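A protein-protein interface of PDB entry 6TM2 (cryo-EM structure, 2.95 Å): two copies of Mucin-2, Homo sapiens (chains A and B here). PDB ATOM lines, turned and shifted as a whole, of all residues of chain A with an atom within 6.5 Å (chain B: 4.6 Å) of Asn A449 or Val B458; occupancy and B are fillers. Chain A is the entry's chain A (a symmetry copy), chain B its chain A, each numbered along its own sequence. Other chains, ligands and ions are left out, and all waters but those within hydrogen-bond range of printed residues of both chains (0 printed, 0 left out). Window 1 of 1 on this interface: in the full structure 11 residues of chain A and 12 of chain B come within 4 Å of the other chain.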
ATOM      1  N   LYS A 435     -21.397  20.337  -7.579  1.00  0.00           N
ATOM      2  CA  LYS A 435     -20.963  20.079  -6.214  1.00  0.00           C
ATOM      3  C   LYS A 435     -19.790  20.953  -5.790  1.00  0.00           C
ATOM      4  O   LYS A 435     -19.477  21.002  -4.596  1.00  0.00           O
ATOM      5  CB  LYS A 435     -20.584  18.603  -6.049  1.00  0.00           C
ATOM      6  N   ASN A 436     -19.141  21.635  -6.730  1.00  0.00           N
ATOM      7  CA  ASN A 436     -18.032  22.535  -6.448  1.00  0.00           C
ATOM      8  C   ASN A 436     -18.454  23.955  -6.794  1.00  0.00           C
ATOM      9  O   ASN A 436     -18.809  24.233  -7.944  1.00  0.00           O
ATOM     10  CB  ASN A 436     -16.789  22.141  -7.245  1.00  0.00           C
ATOM     11  CG  ASN A 436     -16.155  20.861  -6.746  1.00  0.00           C
ATOM     12  OD1 ASN A 436     -16.031  20.645  -5.544  1.00  0.00           O
ATOM     13  ND2 ASN A 436     -15.743  20.006  -7.670  1.00  0.00           N
ATOM     14  N   ALA A 437     -18.410  24.846  -5.810  1.00  0.00           N
ATOM     15  CA  ALA A 437     -18.749  26.250  -5.999  1.00  0.00           C
ATOM     16  C   ALA A 437     -17.476  27.075  -5.928  1.00  0.00           C
ATOM     17  O   ALA A 437     -16.741  26.998  -4.938  1.00  0.00           O
ATOM     18  CB  ALA A 437     -19.745  26.721  -4.941  1.00  0.00           C
ATOM     19  N   VAL A 438     -17.217  27.864  -6.968  1.00  0.00           N
ATOM     20  CA  VAL A 438     -16.045  28.728  -7.038  1.00  0.00           C
ATOM     21  C   VAL A 438     -16.540  30.167  -7.069  1.00  0.00           C
ATOM     22  O   VAL A 438     -17.445  30.494  -7.841  1.00  0.00           O
ATOM     23  CB  VAL A 438     -15.189  28.407  -8.278  1.00  0.00           C
ATOM     24  CG1 VAL A 438     -13.968  29.277  -8.326  1.00  0.00           C
ATOM     25  CG2 VAL A 438     -14.802  26.950  -8.300  1.00  0.00           C
ATOM     26  N   VAL A 439     -15.958  31.022  -6.229  1.00  0.00           N
ATOM     27  CA  VAL A 439     -16.429  32.391  -6.036  1.00  0.00           C
ATOM     28  C   VAL A 439     -15.300  33.354  -6.372  1.00  0.00           C
ATOM     29  O   VAL A 439     -14.183  33.206  -5.869  1.00  0.00           O
ATOM     30  CB  VAL A 439     -16.938  32.610  -4.598  1.00  0.00           C
ATOM     31  CG1 VAL A 439     -17.296  34.058  -4.356  1.00  0.00           C
ATOM     32  CG2 VAL A 439     -18.147  31.741  -4.335  1.00  0.00           C
ATOM     33  N   LEU A 447     -12.134  31.794  -3.865  1.00  0.00           N
ATOM     34  CA  LEU A 447     -12.368  30.871  -2.769  1.00  0.00           C
ATOM     35  C   LEU A 447     -13.273  29.728  -3.208  1.00  0.00           C
ATOM     36  O   LEU A 447     -14.328  29.948  -3.806  1.00  0.00           O
ATOM     37  CB  LEU A 447     -12.912  31.619  -1.543  1.00  0.00           C
ATOM     38  CG  LEU A 447     -14.181  32.468  -1.524  1.00  0.00           C
ATOM     39  CD1 LEU A 447     -15.420  31.661  -1.199  1.00  0.00           C
ATOM     40  CD2 LEU A 447     -14.018  33.618  -0.552  1.00  0.00           C
ATOM     41  N   LEU A 448     -12.826  28.509  -2.923  1.00  0.00           N
ATOM     42  CA  LEU A 448     -13.520  27.277  -3.268  1.00  0.00           C
ATOM     43  C   LEU A 448     -14.189  26.706  -2.027  1.00  0.00           C
ATOM     44  O   LEU A 448     -13.500  26.358  -1.062  1.00  0.00           O
ATOM     45  CB  LEU A 448     -12.539  26.260  -3.848  1.00  0.00           C
ATOM     46  CG  LEU A 448     -13.049  24.864  -4.204  1.00  0.00           C
ATOM     47  CD1 LEU A 448     -14.099  24.905  -5.279  1.00  0.00           C
ATOM     48  CD2 LEU A 448     -11.893  23.980  -4.628  1.00  0.00           C
ATOM     49  N   ASN A 449     -15.524  26.603  -2.074  1.00  0.00           N
ATOM     50  CA  ASN A 449     -16.362  26.047  -1.003  1.00  0.00           C
ATOM     51  C   ASN A 449     -16.138  26.777   0.319  1.00  0.00           C
ATOM     52  O   ASN A 449     -15.860  26.166   1.352  1.00  0.00           O
ATOM     53  CB  ASN A 449     -16.146  24.539  -0.862  1.00  0.00           C
ATOM     54  CG  ASN A 449     -16.714  23.760  -2.036  1.00  0.00           C
ATOM     55  OD1 ASN A 449     -17.817  24.038  -2.500  1.00  0.00           O
ATOM     56  ND2 ASN A 449     -15.950  22.797  -2.534  1.00  0.00           N
ATOM     57  N   GLN A 450     -16.232  28.112   0.250  1.00  0.00           N
ATOM     58  CA  GLN A 450     -16.077  29.040   1.376  1.00  0.00           C
ATOM     59  C   GLN A 450     -14.698  28.950   2.026  1.00  0.00           C
ATOM     60  O   GLN A 450     -14.548  29.212   3.221  1.00  0.00           O
ATOM     61  CB  GLN A 450     -17.181  28.856   2.423  1.00  0.00           C
ATOM     62  N   LEU A 451     -13.673  28.603   1.248  1.00  0.00           N
ATOM     63  CA  LEU A 451     -12.309  28.499   1.753  1.00  0.00           C
ATOM     64  C   LEU A 451     -11.351  29.080   0.727  1.00  0.00           C
ATOM     65  O   LEU A 451     -11.459  28.758  -0.458  1.00  0.00           O
ATOM     66  CB  LEU A 451     -11.932  27.042   2.046  1.00  0.00           C
ATOM     67  CG  LEU A 451     -12.664  26.301   3.166  1.00  0.00           C
ATOM     68  CD1 LEU A 451     -12.248  24.842   3.196  1.00  0.00           C
ATOM     69  CD2 LEU A 451     -12.403  26.963   4.507  1.00  0.00           C
ATOM     70  N   PRO B 456      -7.568  24.373   5.909  1.00  0.00           N
ATOM     71  CA  PRO B 456      -8.285  23.230   5.325  1.00  0.00           C
ATOM     72  C   PRO B 456      -8.580  23.344   3.834  1.00  0.00           C
ATOM     73  O   PRO B 456      -8.540  24.434   3.270  1.00  0.00           O
ATOM     74  CB  PRO B 456      -9.600  23.211   6.107  1.00  0.00           C
ATOM     75  CG  PRO B 456      -9.312  23.919   7.362  1.00  0.00           C
ATOM     76  CD  PRO B 456      -8.352  24.996   6.984  1.00  0.00           C
ATOM     77  N   HIS B 457      -8.868  22.203   3.212  1.00  0.00           N
ATOM     78  CA  HIS B 457      -9.146  22.122   1.779  1.00  0.00           C
ATOM     79  C   HIS B 457     -10.239  21.075   1.596  1.00  0.00           C
ATOM     80  O   HIS B 457      -9.949  19.879   1.514  1.00  0.00           O
ATOM     81  CB  HIS B 457      -7.893  21.759   0.994  1.00  0.00           C
ATOM     82  CG  HIS B 457      -8.103  21.678  -0.485  1.00  0.00           C
ATOM     83  ND1 HIS B 457      -8.222  22.792  -1.285  1.00  0.00           N
ATOM     84  CD2 HIS B 457      -8.221  20.610  -1.309  1.00  0.00           C
ATOM     85  CE1 HIS B 457      -8.399  22.416  -2.538  1.00  0.00           C
ATOM     86  NE2 HIS B 457      -8.402  21.097  -2.581  1.00  0.00           N
ATOM     87  N   VAL B 458     -11.488  21.525   1.534  1.00  0.00           N
ATOM     88  CA  VAL B 458     -12.649  20.645   1.455  1.00  0.00           C
ATOM     89  C   VAL B 458     -13.174  20.668   0.028  1.00  0.00           C
ATOM     90  O   VAL B 458     -13.447  21.741  -0.520  1.00  0.00           O
ATOM     91  CB  VAL B 458     -13.739  21.069   2.454  1.00  0.00           C
ATOM     92  CG1 VAL B 458     -14.982  20.216   2.287  1.00  0.00           C
ATOM     93  CG2 VAL B 458     -13.218  20.973   3.874  1.00  0.00           C
ATOM     94  N   THR B 459     -13.308  19.491  -0.572  1.00  0.00           N
ATOM     95  CA  THR B 459     -13.804  19.343  -1.934  1.00  0.00           C
ATOM     96  C   THR B 459     -15.019  18.419  -1.938  1.00  0.00           C
ATOM     97  O   THR B 459     -15.588  18.098  -0.892  1.00  0.00           O
ATOM     98  CB  THR B 459     -12.717  18.808  -2.870  1.00  0.00           C
ATOM     99  OG1 THR B 459     -12.286  17.519  -2.418  1.00  0.00           O
ATOM    100  CG2 THR B 459     -11.527  19.756  -2.931  1.00  0.00           C
ATOM    101  N   PHE B 462     -13.075  14.503  -1.543  1.00  0.00           N
ATOM    102  CA  PHE B 462     -12.242  14.310  -0.365  1.00  0.00           C
ATOM    103  C   PHE B 462     -12.061  15.646   0.340  1.00  0.00           C
ATOM    104  O   PHE B 462     -12.493  16.693  -0.145  1.00  0.00           O
ATOM    105  CB  PHE B 462     -10.884  13.678  -0.721  1.00  0.00           C
ATOM    106  CG  PHE B 462      -9.991  14.550  -1.561  1.00  0.00           C
ATOM    107  CD1 PHE B 462     -10.100  14.544  -2.940  1.00  0.00           C
ATOM    108  CD2 PHE B 462      -8.996  15.318  -0.977  1.00  0.00           C
ATOM    109  CE1 PHE B 462      -9.275  15.332  -3.716  1.00  0.00           C
ATOM    110  CE2 PHE B 462      -8.169  16.105  -1.744  1.00  0.00           C
ATOM    111  CZ  PHE B 462      -8.307  16.111  -3.115  1.00  0.00           C
ATOM    112  N   SER B 463     -11.401  15.594   1.496  1.00  0.00           N
ATOM    113  CA  SER B 463     -11.107  16.789   2.272  1.00  0.00           C
ATOM    114  C   SER B 463      -9.912  16.508   3.169  1.00  0.00           C
ATOM    115  O   SER B 463      -9.783  15.409   3.709  1.00  0.00           O
ATOM    116  CB  SER B 463     -12.312  17.219   3.112  1.00  0.00           C
ATOM    117  OG  SER B 463     -12.603  16.261   4.111  1.00  0.00           O
ATOM    118  N   PHE B 465      -7.660  17.984   6.470  1.00  0.00           N
ATOM    119  CA  PHE B 465      -7.712  18.858   7.634  1.00  0.00           C
ATOM    120  C   PHE B 465      -6.359  18.878   8.332  1.00  0.00           C
ATOM    121  O   PHE B 465      -5.476  18.070   8.048  1.00  0.00           O
ATOM    122  CB  PHE B 465      -8.786  18.402   8.622  1.00  0.00           C
ATOM    123  CG  PHE B 465     -10.168  18.425   8.060  1.00  0.00           C
ATOM    124  CD1 PHE B 465     -10.858  19.615   7.930  1.00  0.00           C
ATOM    125  CD2 PHE B 465     -10.789  17.246   7.683  1.00  0.00           C
ATOM    126  CE1 PHE B 465     -12.131  19.632   7.413  1.00  0.00           C
ATOM    127  CE2 PHE B 465     -12.063  17.256   7.171  1.00  0.00           C
ATOM    128  CZ  PHE B 465     -12.734  18.450   7.035  1.00  0.00           C
ATOM    129  N   HIS B 667     -17.986  20.600   7.374  1.00  0.00           N
ATOM    130  CA  HIS B 667     -16.723  19.917   7.654  1.00  0.00           C
ATOM    131  C   HIS B 667     -16.589  19.649   9.157  1.00  0.00           C
ATOM    132  O   HIS B 667     -16.100  20.472   9.938  1.00  0.00           O
ATOM    133  CB  HIS B 667     -15.531  20.709   7.056  1.00  0.00           C
ATOM    134  CG  HIS B 667     -15.385  22.115   7.557  1.00  0.00           C
ATOM    135  ND1 HIS B 667     -14.689  22.423   8.707  1.00  0.00           N
ATOM    136  CD2 HIS B 667     -15.817  23.293   7.051  1.00  0.00           C
ATOM    137  CE1 HIS B 667     -14.710  23.730   8.894  1.00  0.00           C
ATOM    138  NE2 HIS B 667     -15.388  24.282   7.905  1.00  0.00           N
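ND2 of Asn A449 lies within hydrogen-bond range of O of Val B458, at 3.4 Å.
Of the 10 printed residues of chain A, 2 touch a printed residue of chain B. Printed residues of chain A that touch a printed residue of chain B: Asn A449 and Leu A451. Among the printed residues, no Asp or Glu carboxylate lies within 4 Å of a Lys or Arg side-chain nitrogen of the other chain.
Among the printed residues, merely in contact across the chains: Leu A451 with Pro B456 (3.7 Å) and Leu A451 with Val B458 (3.8 Å).
N of Asn A449 is in hydrogen-bond range of O of Ala A437.
No position is printed for both chains. Of the 3 pairs that touch across the chains among the printed residues, none has its exchanged pair printed and touching as well.
Of the printed residues of chain B, Asn A449 touches Val B458 (3.4 Å). Of the printed residues of chain B, Leu A451 touches Pro B456 and Val B458. Printed residues of chain A within 4 Å of Pro B456: Leu A451.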
